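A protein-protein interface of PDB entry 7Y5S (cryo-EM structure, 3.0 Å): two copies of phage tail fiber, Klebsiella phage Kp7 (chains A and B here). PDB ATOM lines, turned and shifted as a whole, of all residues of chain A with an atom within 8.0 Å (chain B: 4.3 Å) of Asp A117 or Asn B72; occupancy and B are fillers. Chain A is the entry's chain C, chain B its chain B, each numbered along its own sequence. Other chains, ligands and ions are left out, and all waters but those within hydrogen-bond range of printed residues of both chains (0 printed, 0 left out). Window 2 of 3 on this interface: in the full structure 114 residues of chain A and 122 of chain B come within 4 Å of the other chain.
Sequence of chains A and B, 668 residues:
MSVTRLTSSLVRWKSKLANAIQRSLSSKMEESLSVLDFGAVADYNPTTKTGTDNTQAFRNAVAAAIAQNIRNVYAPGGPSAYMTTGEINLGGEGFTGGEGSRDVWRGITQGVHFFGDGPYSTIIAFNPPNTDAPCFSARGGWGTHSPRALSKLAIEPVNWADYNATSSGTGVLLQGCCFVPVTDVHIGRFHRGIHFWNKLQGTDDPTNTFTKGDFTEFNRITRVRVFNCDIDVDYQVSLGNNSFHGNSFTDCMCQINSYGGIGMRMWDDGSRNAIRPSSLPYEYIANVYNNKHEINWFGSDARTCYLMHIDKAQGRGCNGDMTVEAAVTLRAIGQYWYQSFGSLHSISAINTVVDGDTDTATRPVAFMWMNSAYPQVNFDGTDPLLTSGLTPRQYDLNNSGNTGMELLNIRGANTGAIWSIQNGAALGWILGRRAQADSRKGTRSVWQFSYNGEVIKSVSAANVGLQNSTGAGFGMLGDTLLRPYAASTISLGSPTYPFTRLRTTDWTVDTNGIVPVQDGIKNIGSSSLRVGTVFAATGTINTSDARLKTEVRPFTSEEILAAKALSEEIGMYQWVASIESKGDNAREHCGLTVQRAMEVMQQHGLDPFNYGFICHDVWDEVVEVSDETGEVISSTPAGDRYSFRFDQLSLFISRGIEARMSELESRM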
ATOM      1  N   TYR A  74     -10.986  -6.376  12.641  1.00  0.00           N
ATOM      2  CA  TYR A  74     -10.451  -7.413  11.766  1.00  0.00           C
ATOM      3  C   TYR A  74     -10.975  -8.773  12.206  1.00  0.00           C
ATOM      4  O   TYR A  74     -10.910  -9.114  13.391  1.00  0.00           O
ATOM      5  CB  TYR A  74      -8.922  -7.393  11.786  1.00  0.00           C
ATOM      6  CG  TYR A  74      -8.265  -8.451  10.929  1.00  0.00           C
ATOM      7  CD1 TYR A  74      -8.734  -8.732   9.653  1.00  0.00           C
ATOM      8  CD2 TYR A  74      -7.170  -9.165  11.397  1.00  0.00           C
ATOM      9  CE1 TYR A  74      -8.132  -9.698   8.869  1.00  0.00           C
ATOM     10  CE2 TYR A  74      -6.563 -10.130  10.621  1.00  0.00           C
ATOM     11  CZ  TYR A  74      -7.047 -10.392   9.359  1.00  0.00           C
ATOM     12  OH  TYR A  74      -6.439 -11.355   8.588  1.00  0.00           O
ATOM     13  N   ALA A  75     -11.499  -9.538  11.254  1.00  0.00           N
ATOM     14  CA  ALA A  75     -11.993 -10.891  11.509  1.00  0.00           C
ATOM     15  C   ALA A  75     -11.193 -11.877  10.673  1.00  0.00           C
ATOM     16  O   ALA A  75     -11.484 -12.061   9.478  1.00  0.00           O
ATOM     17  CB  ALA A  75     -13.483 -10.999  11.189  1.00  0.00           C
ATOM     18  N   PRO A  76     -10.182 -12.528  11.242  1.00  0.00           N
ATOM     19  CA  PRO A  76      -9.365 -13.458  10.454  1.00  0.00           C
ATOM     20  C   PRO A  76     -10.115 -14.741  10.130  1.00  0.00           C
ATOM     21  O   PRO A  76     -11.110 -15.099  10.765  1.00  0.00           O
ATOM     22  CB  PRO A  76      -8.163 -13.732  11.362  1.00  0.00           C
ATOM     23  CG  PRO A  76      -8.661 -13.467  12.735  1.00  0.00           C
ATOM     24  CD  PRO A  76      -9.690 -12.382  12.621  1.00  0.00           C
ATOM     25  N   GLY A  77      -9.607 -15.439   9.118  1.00  0.00           N
ATOM     26  CA  GLY A  77     -10.193 -16.682   8.656  1.00  0.00           C
ATOM     27  C   GLY A  77      -9.772 -17.892   9.466  1.00  0.00           C
ATOM     28  O   GLY A  77      -8.913 -18.665   9.033  1.00  0.00           O
ATOM     29  N   GLY A  78     -10.362 -18.061  10.649  1.00  0.00           N
ATOM     30  CA  GLY A  78     -10.018 -19.152  11.529  1.00  0.00           C
ATOM     31  C   GLY A  78     -10.378 -20.518  10.976  1.00  0.00           C
ATOM     32  O   GLY A  78     -10.734 -20.669   9.803  1.00  0.00           O
ATOM     33  N   TYR A  82     -17.528 -18.176  12.141  1.00  0.00           N
ATOM     34  CA  TYR A  82     -17.936 -17.521  13.374  1.00  0.00           C
ATOM     35  C   TYR A  82     -19.453 -17.584  13.482  1.00  0.00           C
ATOM     36  O   TYR A  82     -20.163 -17.107  12.590  1.00  0.00           O
ATOM     37  CB  TYR A  82     -17.465 -16.067  13.406  1.00  0.00           C
ATOM     38  CG  TYR A  82     -15.963 -15.897  13.392  1.00  0.00           C
ATOM     39  CD1 TYR A  82     -15.238 -15.870  14.576  1.00  0.00           C
ATOM     40  CD2 TYR A  82     -15.273 -15.749  12.198  1.00  0.00           C
ATOM     41  CE1 TYR A  82     -13.866 -15.712  14.569  1.00  0.00           C
ATOM     42  CE2 TYR A  82     -13.902 -15.589  12.181  1.00  0.00           C
ATOM     43  CZ  TYR A  82     -13.203 -15.571  13.368  1.00  0.00           C
ATOM     44  OH  TYR A  82     -11.836 -15.410  13.353  1.00  0.00           O
ATOM     45  N   PHE A 115     -13.847  -5.724   8.210  1.00  0.00           N
ATOM     46  CA  PHE A 115     -13.253  -6.421   7.080  1.00  0.00           C
ATOM     47  C   PHE A 115     -12.646  -7.731   7.557  1.00  0.00           C
ATOM     48  O   PHE A 115     -12.283  -7.883   8.726  1.00  0.00           O
ATOM     49  CB  PHE A 115     -12.192  -5.562   6.375  1.00  0.00           C
ATOM     50  CG  PHE A 115     -10.948  -5.341   7.188  1.00  0.00           C
ATOM     51  CD1 PHE A 115     -10.921  -4.389   8.193  1.00  0.00           C
ATOM     52  CD2 PHE A 115      -9.803  -6.079   6.941  1.00  0.00           C
ATOM     53  CE1 PHE A 115      -9.778  -4.183   8.941  1.00  0.00           C
ATOM     54  CE2 PHE A 115      -8.657  -5.877   7.684  1.00  0.00           C
ATOM     55  CZ  PHE A 115      -8.645  -4.926   8.685  1.00  0.00           C
ATOM     56  N   GLY A 116     -12.544  -8.681   6.632  1.00  0.00           N
ATOM     57  CA  GLY A 116     -11.982  -9.981   6.939  1.00  0.00           C
ATOM     58  C   GLY A 116     -10.698 -10.271   6.190  1.00  0.00           C
ATOM     59  O   GLY A 116      -9.790  -9.436   6.150  1.00  0.00           O
ATOM     60  N   ASP A 117     -10.612 -11.459   5.589  1.00  0.00           N
ATOM     61  CA  ASP A 117      -9.427 -11.876   4.855  1.00  0.00           C
ATOM     62  C   ASP A 117      -9.656 -12.048   3.362  1.00  0.00           C
ATOM     63  O   ASP A 117      -8.693 -11.958   2.595  1.00  0.00           O
ATOM     64  CB  ASP A 117      -8.885 -13.195   5.423  1.00  0.00           C
ATOM     65  CG  ASP A 117      -7.739 -12.987   6.389  1.00  0.00           C
ATOM     66  OD1 ASP A 117      -7.271 -11.835   6.518  1.00  0.00           O
ATOM     67  OD2 ASP A 117      -7.305 -13.971   7.022  1.00  0.00           O
ATOM     68  N   GLY A 118     -10.891 -12.292   2.933  1.00  0.00           N
ATOM     69  CA  GLY A 118     -11.192 -12.478   1.534  1.00  0.00           C
ATOM     70  C   GLY A 118     -12.669 -12.709   1.299  1.00  0.00           C
ATOM     71  O   GLY A 118     -13.461 -12.811   2.240  1.00  0.00           O
ATOM     72  N   PRO A 119     -13.070 -12.794   0.027  1.00  0.00           N
ATOM     73  CA  PRO A 119     -14.494 -13.012  -0.276  1.00  0.00           C
ATOM     74  C   PRO A 119     -15.057 -14.284   0.332  1.00  0.00           C
ATOM     75  O   PRO A 119     -16.223 -14.297   0.748  1.00  0.00           O
ATOM     76  CB  PRO A 119     -14.517 -13.064  -1.810  1.00  0.00           C
ATOM     77  CG  PRO A 119     -13.296 -12.312  -2.232  1.00  0.00           C
ATOM     78  CD  PRO A 119     -12.263 -12.631  -1.193  1.00  0.00           C
ATOM     79  N   TYR A 120     -14.265 -15.356   0.402  1.00  0.00           N
ATOM     80  CA  TYR A 120     -14.699 -16.602   1.020  1.00  0.00           C
ATOM     81  C   TYR A 120     -13.697 -17.122   2.043  1.00  0.00           C
ATOM     82  O   TYR A 120     -13.814 -18.275   2.476  1.00  0.00           O
ATOM     83  CB  TYR A 120     -14.954 -17.670  -0.050  1.00  0.00           C
ATOM     84  CG  TYR A 120     -15.970 -18.712   0.356  1.00  0.00           C
ATOM     85  CD1 TYR A 120     -17.287 -18.361   0.626  1.00  0.00           C
ATOM     86  CD2 TYR A 120     -15.614 -20.049   0.460  1.00  0.00           C
ATOM     87  CE1 TYR A 120     -18.216 -19.312   0.997  1.00  0.00           C
ATOM     88  CE2 TYR A 120     -16.536 -21.007   0.827  1.00  0.00           C
ATOM     89  CZ  TYR A 120     -17.835 -20.635   1.095  1.00  0.00           C
ATOM     90  OH  TYR A 120     -18.756 -21.588   1.462  1.00  0.00           O
ATOM     91  N   SER A 121     -12.719 -16.311   2.440  1.00  0.00           N
ATOM     92  CA  SER A 121     -11.750 -16.754   3.434  1.00  0.00           C
ATOM     93  C   SER A 121     -12.359 -16.784   4.831  1.00  0.00           C
ATOM     94  O   SER A 121     -12.080 -17.699   5.612  1.00  0.00           O
ATOM     95  CB  SER A 121     -10.522 -15.843   3.406  1.00  0.00           C
ATOM     96  OG  SER A 121      -9.867 -15.916   2.152  1.00  0.00           O
ATOM     97  N   THR A 122     -13.185 -15.797   5.158  1.00  0.00           N
ATOM     98  CA  THR A 122     -13.845 -15.715   6.455  1.00  0.00           C
ATOM     99  C   THR A 122     -15.335 -15.968   6.281  1.00  0.00           C
ATOM    100  O   THR A 122     -15.968 -15.401   5.384  1.00  0.00           O
ATOM    101  CB  THR A 122     -13.600 -14.356   7.114  1.00  0.00           C
ATOM    102  OG1 THR A 122     -14.374 -13.346   6.453  1.00  0.00           O
ATOM    103  CG2 THR A 122     -12.128 -13.999   7.046  1.00  0.00           C
ATOM    104  N   ILE A 123     -15.888 -16.825   7.136  1.00  0.00           N
ATOM    105  CA  ILE A 123     -17.273 -17.267   7.041  1.00  0.00           C
ATOM    106  C   ILE A 123     -17.996 -16.904   8.329  1.00  0.00           C
ATOM    107  O   ILE A 123     -17.497 -17.177   9.427  1.00  0.00           O
ATOM    108  CB  ILE A 123     -17.368 -18.780   6.773  1.00  0.00           C
ATOM    109  CG1 ILE A 123     -16.492 -19.168   5.584  1.00  0.00           C
ATOM    110  CG2 ILE A 123     -18.804 -19.184   6.500  1.00  0.00           C
ATOM    111  CD1 ILE A 123     -16.908 -18.494   4.303  1.00  0.00           C
ATOM    112  N   SER A 151     -16.364  -5.381   4.113  1.00  0.00           N
ATOM    113  CA  SER A 151     -15.693  -5.966   2.962  1.00  0.00           C
ATOM    114  C   SER A 151     -15.123  -7.330   3.326  1.00  0.00           C
ATOM    115  O   SER A 151     -14.820  -7.608   4.488  1.00  0.00           O
ATOM    116  CB  SER A 151     -14.581  -5.048   2.439  1.00  0.00           C
ATOM    117  OG  SER A 151     -13.477  -5.034   3.326  1.00  0.00           O
ATOM    118  N   LYS A 152     -14.983  -8.174   2.302  1.00  0.00           N
ATOM    119  CA  LYS A 152     -14.204  -9.412   2.366  1.00  0.00           C
ATOM    120  C   LYS A 152     -14.728 -10.372   3.437  1.00  0.00           C
ATOM    121  O   LYS A 152     -14.032 -10.711   4.397  1.00  0.00           O
ATOM    122  CB  LYS A 152     -12.721  -9.098   2.588  1.00  0.00           C
ATOM    123  CG  LYS A 152     -12.121  -8.182   1.535  1.00  0.00           C
ATOM    124  CD  LYS A 152     -10.622  -8.034   1.721  1.00  0.00           C
ATOM    125  CE  LYS A 152     -10.286  -6.689   2.342  1.00  0.00           C
ATOM    126  NZ  LYS A 152      -8.834  -6.569   2.648  1.00  0.00           N
ATOM    127  N   LEU A 153     -15.968 -10.824   3.247  1.00  0.00           N
ATOM    128  CA  LEU A 153     -16.551 -11.843   4.112  1.00  0.00           C
ATOM    129  C   LEU A 153     -17.839 -12.370   3.487  1.00  0.00           C
ATOM    130  O   LEU A 153     -18.232 -11.979   2.383  1.00  0.00           O
ATOM    131  CB  LEU A 153     -16.778 -11.301   5.532  1.00  0.00           C
ATOM    132  CG  LEU A 153     -17.676 -10.090   5.792  1.00  0.00           C
ATOM    133  CD1 LEU A 153     -19.140 -10.478   5.951  1.00  0.00           C
ATOM    134  CD2 LEU A 153     -17.177  -9.337   7.017  1.00  0.00           C
ATOM    135  N   ASP A 184     -16.663  -7.071  -2.251  1.00  0.00           N
ATOM    136  CA  ASP A 184     -16.087  -8.416  -2.240  1.00  0.00           C
ATOM    137  C   ASP A 184     -16.671  -9.268  -1.107  1.00  0.00           C
ATOM    138  O   ASP A 184     -15.958  -9.785  -0.246  1.00  0.00           O
ATOM    139  CB  ASP A 184     -14.556  -8.346  -2.137  1.00  0.00           C
ATOM    140  CG  ASP A 184     -13.871  -8.489  -3.481  1.00  0.00           C
ATOM    141  OD1 ASP A 184     -14.568  -8.779  -4.474  1.00  0.00           O
ATOM    142  OD2 ASP A 184     -12.637  -8.310  -3.544  1.00  0.00           O
ATOM    143  N   ALA B  65      -2.005 -22.846   4.117  1.00  0.00           N
ATOM    144  CA  ALA B  65      -3.191 -22.002   4.214  1.00  0.00           C
ATOM    145  C   ALA B  65      -4.460 -22.806   3.965  1.00  0.00           C
ATOM    146  O   ALA B  65      -5.467 -22.619   4.657  1.00  0.00           O
ATOM    147  CB  ALA B  65      -3.084 -20.840   3.228  1.00  0.00           C
ATOM    148  N   ILE B  70      -7.143 -21.087   6.758  1.00  0.00           N
ATOM    149  CA  ILE B  70      -6.786 -19.667   6.741  1.00  0.00           C
ATOM    150  C   ILE B  70      -6.448 -19.330   5.289  1.00  0.00           C
ATOM    151  O   ILE B  70      -5.290 -19.304   4.873  1.00  0.00           O
ATOM    152  CB  ILE B  70      -5.658 -19.346   7.727  1.00  0.00           C
ATOM    153  CG1 ILE B  70      -5.362 -17.842   7.757  1.00  0.00           C
ATOM    154  CG2 ILE B  70      -4.418 -20.233   7.512  1.00  0.00           C
ATOM    155  CD1 ILE B  70      -4.504 -17.413   8.925  1.00  0.00           C
ATOM    156  N   ARG B  71      -7.491 -19.047   4.509  1.00  0.00           N
ATOM    157  CA  ARG B  71      -7.383 -18.990   3.051  1.00  0.00           C
ATOM    158  C   ARG B  71      -6.879 -17.617   2.604  1.00  0.00           C
ATOM    159  O   ARG B  71      -7.583 -16.825   1.975  1.00  0.00           O
ATOM    160  CB  ARG B  71      -8.726 -19.330   2.416  1.00  0.00           C
ATOM    161  CG  ARG B  71      -9.396 -20.549   3.029  1.00  0.00           C
ATOM    162  CD  ARG B  71     -10.902 -20.530   2.822  1.00  0.00           C
ATOM    163  NE  ARG B  71     -11.532 -21.747   3.321  1.00  0.00           N
ATOM    164  CZ  ARG B  71     -12.840 -21.958   3.349  1.00  0.00           C
ATOM    165  NH1 ARG B  71     -13.696 -21.048   2.916  1.00  0.00           N
ATOM    166  NH2 ARG B  71     -13.301 -23.110   3.826  1.00  0.00           N
ATOM    167  N   ASN B  72      -5.617 -17.351   2.941  1.00  0.00           N
ATOM    168  CA  ASN B  72      -4.933 -16.152   2.478  1.00  0.00           C
ATOM    169  C   ASN B  72      -3.437 -16.311   2.713  1.00  0.00           C
ATOM    170  O   ASN B  72      -3.019 -16.822   3.756  1.00  0.00           O
ATOM    171  CB  ASN B  72      -5.451 -14.891   3.185  1.00  0.00           C
ATOM    172  CG  ASN B  72      -5.272 -14.948   4.687  1.00  0.00           C
ATOM    173  OD1 ASN B  72      -5.806 -15.833   5.351  1.00  0.00           O
ATOM    174  ND2 ASN B  72      -4.517 -14.000   5.228  1.00  0.00           N
ATOM    175  N   VAL B  73      -2.645 -15.879   1.736  1.00  0.00           N
ATOM    176  CA  VAL B  73      -1.189 -15.871   1.833  1.00  0.00           C
ATOM    177  C   VAL B  73      -0.699 -14.468   1.510  1.00  0.00           C
ATOM    178  O   VAL B  73      -1.103 -13.883   0.497  1.00  0.00           O
ATOM    179  CB  VAL B  73      -0.541 -16.906   0.893  1.00  0.00           C
ATOM    180  CG1 VAL B  73       0.970 -16.727   0.863  1.00  0.00           C
ATOM    181  CG2 VAL B  73      -0.892 -18.315   1.338  1.00  0.00           C
ATOM    182  N   VAL B 112      -7.046 -20.147  -1.996  1.00  0.00           N
ATOM    183  CA  VAL B 112      -6.195 -19.191  -1.292  1.00  0.00           C
ATOM    184  C   VAL B 112      -6.368 -17.818  -1.927  1.00  0.00           C
ATOM    185  O   VAL B 112      -6.419 -17.691  -3.156  1.00  0.00           O
ATOM    186  CB  VAL B 112      -4.708 -19.609  -1.321  1.00  0.00           C
ATOM    187  CG1 VAL B 112      -3.842 -18.541  -0.679  1.00  0.00           C
ATOM    188  CG2 VAL B 112      -4.504 -20.933  -0.610  1.00  0.00           C
ATOM    189  N   HIS B 113      -6.459 -16.788  -1.086  1.00  0.00           N
ATOM    190  CA  HIS B 113      -6.446 -15.394  -1.528  1.00  0.00           C
ATOM    191  C   HIS B 113      -5.009 -14.893  -1.447  1.00  0.00           C
ATOM    192  O   HIS B 113      -4.514 -14.563  -0.366  1.00  0.00           O
ATOM    193  CB  HIS B 113      -7.383 -14.542  -0.677  1.00  0.00           C
ATOM    194  CG  HIS B 113      -7.294 -13.074  -0.967  1.00  0.00           C
ATOM    195  ND1 HIS B 113      -7.043 -12.578  -2.229  1.00  0.00           N
ATOM    196  CD2 HIS B 113      -7.421 -11.995  -0.158  1.00  0.00           C
ATOM    197  CE1 HIS B 113      -7.023 -11.257  -2.184  1.00  0.00           C
ATOM    198  NE2 HIS B 113      -7.250 -10.880  -0.939  1.00  0.00           N
ATOM    199  N   PHE B 115      -2.388 -12.151  -1.941  1.00  0.00           N
ATOM    200  CA  PHE B 115      -2.304 -10.703  -2.055  1.00  0.00           C
ATOM    201  C   PHE B 115      -0.935 -10.239  -1.582  1.00  0.00           C
ATOM    202  O   PHE B 115      -0.268 -10.906  -0.788  1.00  0.00           O
ATOM    203  CB  PHE B 115      -3.413 -10.004  -1.255  1.00  0.00           C
ATOM    204  CG  PHE B 115      -3.262 -10.127   0.234  1.00  0.00           C
ATOM    205  CD1 PHE B 115      -3.644 -11.285   0.889  1.00  0.00           C
ATOM    206  CD2 PHE B 115      -2.746  -9.080   0.980  1.00  0.00           C
ATOM    207  CE1 PHE B 115      -3.508 -11.399   2.259  1.00  0.00           C
ATOM    208  CE2 PHE B 115      -2.608  -9.188   2.349  1.00  0.00           C
ATOM    209  CZ  PHE B 115      -2.989 -10.349   2.990  1.00  0.00           C
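N of Ile B70 sits at hydrogen-bond distance from O of Ala B65, at 3.1 Å. N of His B113 sits at hydrogen-bond distance from O of Arg B71 (3.3 Å). The backbone NH (N) of Val B73 lies within hydrogen-bond range of the backbone carbonyl oxygen (O) of His B113 (3.1 Å). OH of Tyr A74 sits close to OD2 of Asp A117, at 3.2 Å. The side-chain carboxylate (OD2) of Asp A117 is in hydrogen-bond range of the backbone NH (N) of Gly A77, at 3.4 Å.
Among the printed residues, merely in contact across the chains: Gly A77 with Ile B70 (3.3 Å) and Asp A117 with His B113 (3.0 Å).
Printed residues of chain B that touch a printed residue of chain A: Ile B70, Arg B71, Asn B72 and His B113. Among the printed residues, 5 pairs touch across the chains. Among the printed residues, no Asp or Glu carboxylate lies within 4 Å of a Lys or Arg side-chain nitrogen of the other chain.
Tyr A82 touches none of the printed residues of chain B. Of chain B, only Asn B72 and His B113 come within 4 Å of Asp A117. Of the printed residues of chain B, Tyr A120 touches Arg B71 (2.8 Å). Of the printed residues of chain A, Ile B70 touches Gly A77. Of chain A, only Asp A117 (2.9 Å) comes within 4 Å of Asn B72. The nearest printed residue of chain B that does not touch Asp A117 is Ile B70 (4.4 Å). The nearest printed residue of chain B that does not touch Ser A121 is His B113 (4.01 Å).
1 position is printed for both chains.
The guanidinium group (NH1) of Arg B71 is in hydrogen-bond range of the backbone carbonyl oxygen (O) of Tyr A120 (2.8 Å). O of Arg B71 sits at hydrogen-bond distance from OG of Ser A121 (2.5 Å). OD1 of Asn B72 lies close to OD2 of Asp A117.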
